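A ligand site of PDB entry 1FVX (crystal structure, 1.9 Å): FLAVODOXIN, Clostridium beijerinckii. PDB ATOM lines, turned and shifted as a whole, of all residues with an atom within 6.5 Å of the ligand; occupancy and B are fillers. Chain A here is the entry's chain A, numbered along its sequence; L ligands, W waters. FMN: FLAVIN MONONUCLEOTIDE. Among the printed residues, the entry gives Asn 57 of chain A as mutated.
Water W3 lies within hydrogen-bond range of the side-chain amide oxygen (OD1) of Asn 119, an oxygen (O3') of the ligand and the side-chain amide oxygen (OD1) of Asn 11.
Water W4 lies within hydrogen-bond range of the side-chain carboxylate of Glu 59 (2.9 Å), the backbone NH of Gly 93 (2.9 Å), an oxygen (O2) of the ligand (3.2 Å) and the backbone NH of Asp 92 (3.5 Å).
Water W1 lies within hydrogen-bond range of the indole nitrogen of Trp 90 (2.7 Å), the side-chain carboxylate of Asp 58 (2.7 Å) and an oxygen (O4) of the ligand (3.2 Å).
N of Thr 9 lies within hydrogen-bond range of O3P of the ligand (2.7 Å).
An oxygen (O3P) of the ligand sits at hydrogen-bond distance from the side-chain hydroxyl (OG1) of Thr 9 (2.6 Å).
An oxygen (O1P) of the ligand sits at hydrogen-bond distance from the backbone NH (N) of Gly 8, at 2.7 Å.
An oxygen (O3P) of the ligand lies within hydrogen-bond range of the backbone NH (N) of Asn 11 (3.0 Å).
OD1 of Asn 11 sits at hydrogen-bond distance from O4' of the ligand (2.7 Å).
The side-chain hydroxyl (OG) of Ser 7 sits at hydrogen-bond distance from an oxygen (O2P) of the ligand.
N of Ala 55 lies within hydrogen-bond range of O2' of the ligand, at 3.4 Å.
O of Ala 55 is in hydrogen-bond range of O2' of the ligand (2.7 Å).
The backbone NH (N) of Gly 91 is in hydrogen-bond range of an oxygen (O2) of the ligand (2.7 Å).
The backbone NH of Thr 12 is in hydrogen-bond range of an oxygen (O2P) of the ligand (2.8 Å).
O2P of the ligand is in hydrogen-bond range of OG1 of Thr 12.
The backbone NH (N) of Glu 59 is in hydrogen-bond range of an oxygen (O4) of the ligand, 3.1 Å away.
The side-chain carboxylate (OE2) of Glu 59 is in hydrogen-bond range of a nitrogen (N3) of the ligand (2.8 Å).
The side-chain hydroxyl (OG) of Ser 54 sits at hydrogen-bond distance from an oxygen (O1P) of the ligand.
An oxygen (O4') of the ligand sits at hydrogen-bond distance from the side-chain hydroxyl (OG) of Ser 87 (2.9 Å).
N of Gly 10 sits at hydrogen-bond distance from O3P of the ligand.
The backbone NH (N) of Gly 89 sits at hydrogen-bond distance from an oxygen (O2) of the ligand, 3.0 Å away.
The backbone NH (N) of Trp 90 lies within hydrogen-bond range of an oxygen (O2) of the ligand, 3.2 Å away.
The backbone NH of Asn 57 lies within hydrogen-bond range of a nitrogen (N5) of the ligand.
N of Asn 11 is in hydrogen-bond range of OG of Ser 7 (3.4 Å).
The side-chain hydroxyl (OG) of Ser 7 sits at hydrogen-bond distance from the backbone NH (N) of Gly 10.
The backbone NH (N) of Glu 13 lies within hydrogen-bond range of the side-chain hydroxyl (OG) of Ser 7 (3.3 Å).
The backbone carbonyl oxygen of Ser 87 is in hydrogen-bond range of the backbone NH of Ala 55, at 3.1 Å.
O of Ser 54 is in hydrogen-bond range of NE1 of Trp 95 (3.5 Å).
The side-chain hydroxyl (OG) of Ser 87 sits at hydrogen-bond distance from the backbone carbonyl oxygen (O) of Asn 119, 2.7 Å away.
The side-chain sulfur (SD) of Met 15 sits close to the backbone NH (N) of Ser 87, 3.8 Å away.
The backbone carbonyl oxygen (O) of Val 117 lies within hydrogen-bond range of the backbone NH (N) of Tyr 88.
O of Met 56 sits close to O4 of the ligand.
Residues that only touch the ligand: Trp 6, Asp 58, Tyr 88 and Asn 119.
Hydrophobic or aromatic side chains that line the ligand: Trp 6, Ala 55, Met 56, Tyr 88 and Trp 90.
The nearest printed residue that does not touch the ligand is Glu 13 (4.5 Å).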
ATOM      1  N   TRP A   6     -13.581   2.873  13.485  1.00  0.00           N
ATOM      2  CA  TRP A   6     -12.486   3.833  13.557  1.00  0.00           C
ATOM      3  C   TRP A   6     -12.303   4.051  15.069  1.00  0.00           C
ATOM      4  O   TRP A   6     -13.301   4.122  15.800  1.00  0.00           O
ATOM      5  CB  TRP A   6     -12.825   5.178  12.879  1.00  0.00           C
ATOM      6  CG  TRP A   6     -11.641   6.116  12.911  1.00  0.00           C
ATOM      7  CD1 TRP A   6     -10.602   6.154  12.020  1.00  0.00           C
ATOM      8  CD2 TRP A   6     -11.303   7.050  13.958  1.00  0.00           C
ATOM      9  NE1 TRP A   6      -9.624   7.025  12.462  1.00  0.00           N
ATOM     10  CE2 TRP A   6     -10.028   7.586  13.641  1.00  0.00           C
ATOM     11  CE3 TRP A   6     -11.949   7.471  15.141  1.00  0.00           C
ATOM     12  CZ2 TRP A   6      -9.378   8.536  14.471  1.00  0.00           C
ATOM     13  CZ3 TRP A   6     -11.299   8.414  15.964  1.00  0.00           C
ATOM     14  CH2 TRP A   6     -10.026   8.924  15.615  1.00  0.00           C
ATOM     15  N   SER A   7     -11.061   4.105  15.533  1.00  0.00           N
ATOM     16  CA  SER A   7     -10.803   4.328  16.957  1.00  0.00           C
ATOM     17  C   SER A   7      -9.528   5.144  17.097  1.00  0.00           C
ATOM     18  O   SER A   7      -8.478   4.770  16.563  1.00  0.00           O
ATOM     19  CB  SER A   7     -10.667   2.991  17.682  1.00  0.00           C
ATOM     20  OG  SER A   7     -10.422   3.178  19.060  1.00  0.00           O
ATOM     21  N   GLY A   8      -9.611   6.247  17.839  1.00  0.00           N
ATOM     22  CA  GLY A   8      -8.461   7.119  18.020  1.00  0.00           C
ATOM     23  C   GLY A   8      -7.514   6.750  19.144  1.00  0.00           C
ATOM     24  O   GLY A   8      -6.330   7.048  19.057  1.00  0.00           O
ATOM     25  N   THR A   9      -8.027   6.167  20.227  1.00  0.00           N
ATOM     26  CA  THR A   9      -7.163   5.774  21.338  1.00  0.00           C
ATOM     27  C   THR A   9      -7.354   4.304  21.716  1.00  0.00           C
ATOM     28  O   THR A   9      -6.698   3.811  22.652  1.00  0.00           O
ATOM     29  CB  THR A   9      -7.366   6.652  22.603  1.00  0.00           C
ATOM     30  OG1 THR A   9      -8.617   6.314  23.237  1.00  0.00           O
ATOM     31  CG2 THR A   9      -7.377   8.131  22.259  1.00  0.00           C
ATOM     32  N   GLY A  10      -8.278   3.619  21.051  1.00  0.00           N
ATOM     33  CA  GLY A  10      -8.508   2.212  21.340  1.00  0.00           C
ATOM     34  C   GLY A  10      -9.797   1.836  22.047  1.00  0.00           C
ATOM     35  O   GLY A  10     -10.082   0.663  22.211  1.00  0.00           O
ATOM     36  N   ASN A  11     -10.608   2.823  22.431  1.00  0.00           N
ATOM     37  CA  ASN A  11     -11.847   2.520  23.140  1.00  0.00           C
ATOM     38  C   ASN A  11     -12.868   1.808  22.269  1.00  0.00           C
ATOM     39  O   ASN A  11     -13.426   0.771  22.665  1.00  0.00           O
ATOM     40  CB  ASN A  11     -12.431   3.776  23.779  1.00  0.00           C
ATOM     41  CG  ASN A  11     -11.549   4.336  24.864  1.00  0.00           C
ATOM     42  OD1 ASN A  11     -11.671   5.498  25.248  1.00  0.00           O
ATOM     43  ND2 ASN A  11     -10.639   3.513  25.366  1.00  0.00           N
ATOM     44  N   THR A  12     -13.122   2.371  21.089  1.00  0.00           N
ATOM     45  CA  THR A  12     -14.052   1.785  20.134  1.00  0.00           C
ATOM     46  C   THR A  12     -13.480   0.465  19.574  1.00  0.00           C
ATOM     47  O   THR A  12     -14.240  -0.468  19.273  1.00  0.00           O
ATOM     48  CB  THR A  12     -14.361   2.773  18.994  1.00  0.00           C
ATOM     49  OG1 THR A  12     -14.909   3.967  19.565  1.00  0.00           O
ATOM     50  CG2 THR A  12     -15.370   2.192  18.014  1.00  0.00           C
ATOM     51  N   GLU A  13     -12.163   0.391  19.449  1.00  0.00           N
ATOM     52  CA  GLU A  13     -11.509  -0.825  18.966  1.00  0.00           C
ATOM     53  C   GLU A  13     -11.771  -1.969  19.951  1.00  0.00           C
ATOM     54  O   GLU A  13     -12.087  -3.087  19.549  1.00  0.00           O
ATOM     55  CB  GLU A  13     -10.000  -0.607  18.818  1.00  0.00           C
ATOM     56  CG  GLU A  13      -9.269  -1.806  18.199  1.00  0.00           C
ATOM     57  CD  GLU A  13      -7.768  -1.629  18.110  1.00  0.00           C
ATOM     58  OE1 GLU A  13      -7.276  -0.480  18.239  1.00  0.00           O
ATOM     59  OE2 GLU A  13      -7.058  -2.636  17.933  1.00  0.00           O
ATOM     60  N   MET A  15     -14.269  -2.161  22.027  1.00  0.00           N
ATOM     61  CA  MET A  15     -15.684  -2.509  21.899  1.00  0.00           C
ATOM     62  C   MET A  15     -15.898  -3.463  20.728  1.00  0.00           C
ATOM     63  O   MET A  15     -16.648  -4.430  20.858  1.00  0.00           O
ATOM     64  CB  MET A  15     -16.558  -1.263  21.656  1.00  0.00           C
ATOM     65  CG  MET A  15     -16.600  -0.274  22.803  1.00  0.00           C
ATOM     66  SD  MET A  15     -17.704   1.112  22.446  1.00  0.00           S
ATOM     67  CE  MET A  15     -17.238   2.093  23.746  1.00  0.00           C
ATOM     68  N   CYS A  53     -17.719   4.076  15.549  1.00  0.00           N
ATOM     69  CA  CYS A  53     -16.856   5.241  15.519  1.00  0.00           C
ATOM     70  C   CYS A  53     -17.118   6.056  16.776  1.00  0.00           C
ATOM     71  O   CYS A  53     -18.284   6.207  17.179  1.00  0.00           O
ATOM     72  CB  CYS A  53     -17.167   6.109  14.298  1.00  0.00           C
ATOM     73  SG  CYS A  53     -16.015   7.500  14.111  1.00  0.00           S
ATOM     74  N   SER A  54     -16.049   6.525  17.402  1.00  0.00           N
ATOM     75  CA  SER A  54     -16.155   7.360  18.604  1.00  0.00           C
ATOM     76  C   SER A  54     -16.661   8.761  18.257  1.00  0.00           C
ATOM     77  O   SER A  54     -16.673   9.164  17.075  1.00  0.00           O
ATOM     78  CB  SER A  54     -14.794   7.464  19.291  1.00  0.00           C
ATOM     79  OG  SER A  54     -13.782   7.818  18.362  1.00  0.00           O
ATOM     80  N   ALA A  55     -17.044   9.512  19.289  1.00  0.00           N
ATOM     81  CA  ALA A  55     -17.552  10.869  19.108  1.00  0.00           C
ATOM     82  C   ALA A  55     -16.412  11.862  18.915  1.00  0.00           C
ATOM     83  O   ALA A  55     -15.505  11.940  19.748  1.00  0.00           O
ATOM     84  CB  ALA A  55     -18.392  11.277  20.316  1.00  0.00           C
ATOM     85  N   MET A  56     -16.424  12.588  17.803  1.00  0.00           N
ATOM     86  CA  MET A  56     -15.408  13.617  17.550  1.00  0.00           C
ATOM     87  C   MET A  56     -16.084  14.995  17.612  1.00  0.00           C
ATOM     88  O   MET A  56     -17.299  15.084  17.744  1.00  0.00           O
ATOM     89  CB  MET A  56     -14.722  13.384  16.207  1.00  0.00           C
ATOM     90  CG  MET A  56     -13.792  12.183  16.201  1.00  0.00           C
ATOM     91  SD  MET A  56     -12.385  12.310  17.348  1.00  0.00           S
ATOM     92  CE  MET A  56     -12.764  10.933  18.470  1.00  0.00           C
ATOM     93  N   ASN A  57     -15.312  16.062  17.527  1.00  0.00           N
ATOM     94  CA  ASN A  57     -15.883  17.408  17.634  1.00  0.00           C
ATOM     95  C   ASN A  57     -16.570  17.954  16.395  1.00  0.00           C
ATOM     96  O   ASN A  57     -16.016  17.939  15.299  1.00  0.00           O
ATOM     97  CB  ASN A  57     -14.838  18.421  18.148  1.00  0.00           C
ATOM     98  CG  ASN A  57     -13.618  18.531  17.237  1.00  0.00           C
ATOM     99  OD1 ASN A  57     -13.179  17.556  16.622  1.00  0.00           O
ATOM    100  ND2 ASN A  57     -13.051  19.730  17.175  1.00  0.00           N
ATOM    101  N   ASP A  58     -17.794  18.443  16.561  1.00  0.00           N
ATOM    102  CA  ASP A  58     -18.447  18.453  17.851  1.00  0.00           C
ATOM    103  C   ASP A  58     -19.683  17.570  17.764  1.00  0.00           C
ATOM    104  O   ASP A  58     -20.700  17.955  17.192  1.00  0.00           O
ATOM    105  CB  ASP A  58     -18.847  19.874  18.235  1.00  0.00           C
ATOM    106  CG  ASP A  58     -19.057  20.010  19.714  1.00  0.00           C
ATOM    107  OD1 ASP A  58     -18.044  20.026  20.448  1.00  0.00           O
ATOM    108  OD2 ASP A  58     -20.236  20.081  20.145  1.00  0.00           O
ATOM    109  N   GLU A  59     -19.561  16.383  18.352  1.00  0.00           N
ATOM    110  CA  GLU A  59     -20.612  15.386  18.308  1.00  0.00           C
ATOM    111  C   GLU A  59     -20.823  14.981  16.850  1.00  0.00           C
ATOM    112  O   GLU A  59     -21.969  14.952  16.371  1.00  0.00           O
ATOM    113  CB  GLU A  59     -21.942  15.877  18.909  1.00  0.00           C
ATOM    114  CG  GLU A  59     -21.892  16.157  20.406  1.00  0.00           C
ATOM    115  CD  GLU A  59     -21.583  14.930  21.248  1.00  0.00           C
ATOM    116  OE1 GLU A  59     -21.881  13.790  20.824  1.00  0.00           O
ATOM    117  OE2 GLU A  59     -21.065  15.120  22.356  1.00  0.00           O
ATOM    118  N   VAL A  60     -19.723  14.700  16.156  1.00  0.00           N
ATOM    119  CA  VAL A  60     -19.779  14.261  14.766  1.00  0.00           C
ATOM    120  C   VAL A  60     -18.919  13.019  14.590  1.00  0.00           C
ATOM    121  O   VAL A  60     -18.129  12.685  15.475  1.00  0.00           O
ATOM    122  CB  VAL A  60     -19.262  15.350  13.782  1.00  0.00           C
ATOM    123  CG1 VAL A  60     -20.098  16.603  13.882  1.00  0.00           C
ATOM    124  CG2 VAL A  60     -17.788  15.650  14.037  1.00  0.00           C
ATOM    125  N   SER A  87     -17.673   4.707  21.302  1.00  0.00           N
ATOM    126  CA  SER A  87     -17.290   5.232  22.609  1.00  0.00           C
ATOM    127  C   SER A  87     -17.365   6.759  22.543  1.00  0.00           C
ATOM    128  O   SER A  87     -17.184   7.362  21.480  1.00  0.00           O
ATOM    129  CB  SER A  87     -15.854   4.814  22.943  1.00  0.00           C
ATOM    130  OG  SER A  87     -15.503   5.177  24.270  1.00  0.00           O
ATOM    131  N   TYR A  88     -17.618   7.389  23.692  1.00  0.00           N
ATOM    132  CA  TYR A  88     -17.709   8.835  23.746  1.00  0.00           C
ATOM    133  C   TYR A  88     -17.154   9.292  25.084  1.00  0.00           C
ATOM    134  O   TYR A  88     -16.873   8.474  25.966  1.00  0.00           O
ATOM    135  CB  TYR A  88     -19.153   9.306  23.550  1.00  0.00           C
ATOM    136  CG  TYR A  88     -20.077   8.908  24.679  1.00  0.00           C
ATOM    137  CD1 TYR A  88     -20.559   7.602  24.772  1.00  0.00           C
ATOM    138  CD2 TYR A  88     -20.446   9.828  25.648  1.00  0.00           C
ATOM    139  CE1 TYR A  88     -21.397   7.222  25.828  1.00  0.00           C
ATOM    140  CE2 TYR A  88     -21.273   9.460  26.705  1.00  0.00           C
ATOM    141  CZ  TYR A  88     -21.753   8.161  26.792  1.00  0.00           C
ATOM    142  OH  TYR A  88     -22.567   7.801  27.829  1.00  0.00           O
ATOM    143  N   GLY A  89     -16.974  10.601  25.232  1.00  0.00           N
ATOM    144  CA  GLY A  89     -16.398  11.109  26.461  1.00  0.00           C
ATOM    145  C   GLY A  89     -17.344  11.906  27.313  1.00  0.00           C
ATOM    146  O   GLY A  89     -18.075  11.355  28.125  1.00  0.00           O
ATOM    147  N   TRP A  90     -17.413  13.194  27.028  1.00  0.00           N
ATOM    148  CA  TRP A  90     -18.216  14.129  27.820  1.00  0.00           C
ATOM    149  C   TRP A  90     -19.647  14.399  27.374  1.00  0.00           C
ATOM    150  O   TRP A  90     -20.406  15.048  28.102  1.00  0.00           O
ATOM    151  CB  TRP A  90     -17.468  15.453  27.941  1.00  0.00           C
ATOM    152  CG  TRP A  90     -17.105  16.049  26.609  1.00  0.00           C
ATOM    153  CD1 TRP A  90     -17.889  16.832  25.820  1.00  0.00           C
ATOM    154  CD2 TRP A  90     -15.846  15.905  25.921  1.00  0.00           C
ATOM    155  NE1 TRP A  90     -17.191  17.195  24.684  1.00  0.00           N
ATOM    156  CE2 TRP A  90     -15.944  16.642  24.728  1.00  0.00           C
ATOM    157  CE3 TRP A  90     -14.655  15.236  26.207  1.00  0.00           C
ATOM    158  CZ2 TRP A  90     -14.889  16.723  23.814  1.00  0.00           C
ATOM    159  CZ3 TRP A  90     -13.609  15.319  25.293  1.00  0.00           C
ATOM    160  CH2 TRP A  90     -13.727  16.058  24.113  1.00  0.00           C
ATOM    161  N   GLY A  91     -20.028  13.934  26.186  1.00  0.00           N
ATOM    162  CA  GLY A  91     -21.355  14.210  25.689  1.00  0.00           C
ATOM    163  C   GLY A  91     -22.409  13.275  26.218  1.00  0.00           C
ATOM    164  O   GLY A  91     -22.153  12.506  27.139  1.00  0.00           O
ATOM    165  N   ASP A  92     -23.603  13.313  25.622  1.00  0.00           N
ATOM    166  CA  ASP A  92     -24.693  12.452  26.028  1.00  0.00           C
ATOM    167  C   ASP A  92     -25.165  11.543  24.891  1.00  0.00           C
ATOM    168  O   ASP A  92     -26.290  11.058  24.908  1.00  0.00           O
ATOM    169  CB  ASP A  92     -25.866  13.271  26.579  1.00  0.00           C
ATOM    170  CG  ASP A  92     -26.499  14.207  25.533  1.00  0.00           C
ATOM    171  OD1 ASP A  92     -26.284  14.032  24.321  1.00  0.00           O
ATOM    172  OD2 ASP A  92     -27.218  15.136  25.959  1.00  0.00           O
ATOM    173  N   GLY A  93     -24.322  11.367  23.880  1.00  0.00           N
ATOM    174  CA  GLY A  93     -24.697  10.507  22.773  1.00  0.00           C
ATOM    175  C   GLY A  93     -25.265  11.200  21.560  1.00  0.00           C
ATOM    176  O   GLY A  93     -25.743  10.536  20.649  1.00  0.00           O
ATOM    177  N   TRP A  95     -23.842  12.478  18.932  1.00  0.00           N
ATOM    178  CA  TRP A  95     -23.243  11.998  17.685  1.00  0.00           C
ATOM    179  C   TRP A  95     -23.874  10.691  17.216  1.00  0.00           C
ATOM    180  O   TRP A  95     -24.049  10.474  16.003  1.00  0.00           O
ATOM    181  CB  TRP A  95     -21.708  11.887  17.809  1.00  0.00           C
ATOM    182  CG  TRP A  95     -21.154  10.484  17.959  1.00  0.00           C
ATOM    183  CD1 TRP A  95     -20.433   9.789  17.012  1.00  0.00           C
ATOM    184  CD2 TRP A  95     -21.233   9.623  19.112  1.00  0.00           C
ATOM    185  NE1 TRP A  95     -20.061   8.563  17.510  1.00  0.00           N
ATOM    186  CE2 TRP A  95     -20.542   8.431  18.789  1.00  0.00           C
ATOM    187  CE3 TRP A  95     -21.820   9.742  20.371  1.00  0.00           C
ATOM    188  CZ2 TRP A  95     -20.406   7.364  19.693  1.00  0.00           C
ATOM    189  CZ3 TRP A  95     -21.694   8.684  21.283  1.00  0.00           C
ATOM    190  CH2 TRP A  95     -20.990   7.507  20.934  1.00  0.00           C
ATOM    191  N   VAL A 117     -20.765   3.536  24.901  1.00  0.00           N
ATOM    192  CA  VAL A 117     -20.093   3.340  26.175  1.00  0.00           C
ATOM    193  C   VAL A 117     -19.157   4.509  26.384  1.00  0.00           C
ATOM    194  O   VAL A 117     -18.486   4.951  25.446  1.00  0.00           O
ATOM    195  CB  VAL A 117     -19.268   2.029  26.176  1.00  0.00           C
ATOM    196  CG1 VAL A 117     -18.390   1.932  27.405  1.00  0.00           C
ATOM    197  CG2 VAL A 117     -20.214   0.821  26.091  1.00  0.00           C
ATOM    198  N   GLN A 118     -19.116   5.008  27.608  1.00  0.00           N
ATOM    199  CA  GLN A 118     -18.250   6.140  27.931  1.00  0.00           C
ATOM    200  C   GLN A 118     -16.828   5.668  28.168  1.00  0.00           C
ATOM    201  O   GLN A 118     -16.595   4.776  28.985  1.00  0.00           O
ATOM    202  CB  GLN A 118     -18.784   6.879  29.154  1.00  0.00           C
ATOM    203  CG  GLN A 118     -18.020   8.147  29.463  1.00  0.00           C
ATOM    204  CD  GLN A 118     -18.643   8.942  30.593  1.00  0.00           C
ATOM    205  OE1 GLN A 118     -19.514   8.453  31.311  1.00  0.00           O
ATOM    206  NE2 GLN A 118     -18.191  10.179  30.755  1.00  0.00           N
ATOM    207  N   ASN A 119     -15.892   6.265  27.434  1.00  0.00           N
ATOM    208  CA  ASN A 119     -14.469   5.913  27.531  1.00  0.00           C
ATOM    209  C   ASN A 119     -14.217   4.411  27.303  1.00  0.00           C
ATOM    210  O   ASN A 119     -14.914   3.803  26.493  1.00  0.00           O
ATOM    211  CB  ASN A 119     -13.885   6.426  28.847  1.00  0.00           C
ATOM    212  CG  ASN A 119     -14.212   7.900  29.090  1.00  0.00           C
ATOM    213  OD1 ASN A 119     -13.813   8.777  28.318  1.00  0.00           O
ATOM    214  ND2 ASN A 119     -14.994   8.165  30.126  1.00  0.00           N
ATOM    215  N   GLU A 120     -13.255   3.801  27.989  1.00  0.00           N
ATOM    216  CA  GLU A 120     -12.983   2.376  27.761  1.00  0.00           C
ATOM    217  C   GLU A 120     -14.101   1.486  28.284  1.00  0.00           C
ATOM    218  O   GLU A 120     -14.659   1.771  29.339  1.00  0.00           O
ATOM    219  CB  GLU A 120     -11.638   1.965  28.382  1.00  0.00           C
ATOM    220  CG  GLU A 120     -11.124   0.604  27.888  1.00  0.00           C
ATOM    221  CD  GLU A 120      -9.730   0.227  28.387  1.00  0.00           C
ATOM    222  OE1 GLU A 120      -8.857   1.126  28.499  1.00  0.00           O
ATOM    223  OE2 GLU A 120      -9.497  -0.974  28.652  1.00  0.00           O
HETATM  224  N1  FMN L   1     -16.603  12.970  23.297  1.00  0.00           N
HETATM  225  C2  FMN L   1     -17.898  13.332  23.299  1.00  0.00           C
HETATM  226  O2  FMN L   1     -18.685  12.798  24.075  1.00  0.00           O
HETATM  227  N3  FMN L   1     -18.325  14.341  22.426  1.00  0.00           N
HETATM  228  C4  FMN L   1     -17.489  15.072  21.612  1.00  0.00           C
HETATM  229  O4  FMN L   1     -17.926  15.986  20.922  1.00  0.00           O
HETATM  230  C4A FMN L   1     -16.068  14.679  21.614  1.00  0.00           C
HETATM  231  N5  FMN L   1     -15.188  15.300  20.851  1.00  0.00           N
HETATM  232  C5A FMN L   1     -13.871  14.883  20.866  1.00  0.00           C
HETATM  233  C6  FMN L   1     -12.912  15.560  20.076  1.00  0.00           C
HETATM  234  C7  FMN L   1     -11.616  15.118  20.011  1.00  0.00           C
HETATM  235  C7M FMN L   1     -10.616  15.871  19.193  1.00  0.00           C
HETATM  236  C8  FMN L   1     -11.224  13.956  20.728  1.00  0.00           C
HETATM  237  C8M FMN L   1      -9.834  13.380  20.662  1.00  0.00           C
HETATM  238  C9  FMN L   1     -12.140  13.307  21.544  1.00  0.00           C
HETATM  239  C9A FMN L   1     -13.468  13.738  21.621  1.00  0.00           C
HETATM  240  N10 FMN L   1     -14.407  13.147  22.455  1.00  0.00           N
HETATM  241  C10 FMN L   1     -15.715  13.577  22.519  1.00  0.00           C
HETATM  242  C1' FMN L   1     -13.948  12.076  23.339  1.00  0.00           C
HETATM  243  C2' FMN L   1     -13.914  10.702  22.656  1.00  0.00           C
HETATM  244  O2' FMN L   1     -15.167  10.436  22.018  1.00  0.00           O
HETATM  245  C3' FMN L   1     -13.652   9.635  23.695  1.00  0.00           C
HETATM  246  O3' FMN L   1     -12.401   9.887  24.332  1.00  0.00           O
HETATM  247  C4' FMN L   1     -13.698   8.168  23.199  1.00  0.00           C
HETATM  248  O4' FMN L   1     -13.515   7.285  24.299  1.00  0.00           O
HETATM  249  C5' FMN L   1     -12.602   7.913  22.159  1.00  0.00           C
HETATM  250  O5' FMN L   1     -12.731   6.591  21.678  1.00  0.00           O
HETATM  251  P   FMN L   1     -11.667   6.033  20.696  1.00  0.00           P
HETATM  252  O1P FMN L   1     -11.358   7.084  19.721  1.00  0.00           O
HETATM  253  O2P FMN L   1     -12.312   4.835  20.151  1.00  0.00           O
HETATM  254  O3P FMN L   1     -10.384   5.649  21.431  1.00  0.00           O
HETATM  255  O   HOH W   1     -18.498  18.568  22.725  1.00  0.00           O
HETATM  256  O   HOH W   2      -9.925   9.426  20.025  1.00  0.00           O
HETATM  257  O   HOH W   3     -11.789   8.536  26.572  1.00  0.00           O
HETATM  258  O   HOH W   4     -21.577  12.028  23.078  1.00  0.00           O
HETATM  259  O   HOH W   5     -10.324  10.336  22.555  1.00  0.00           O
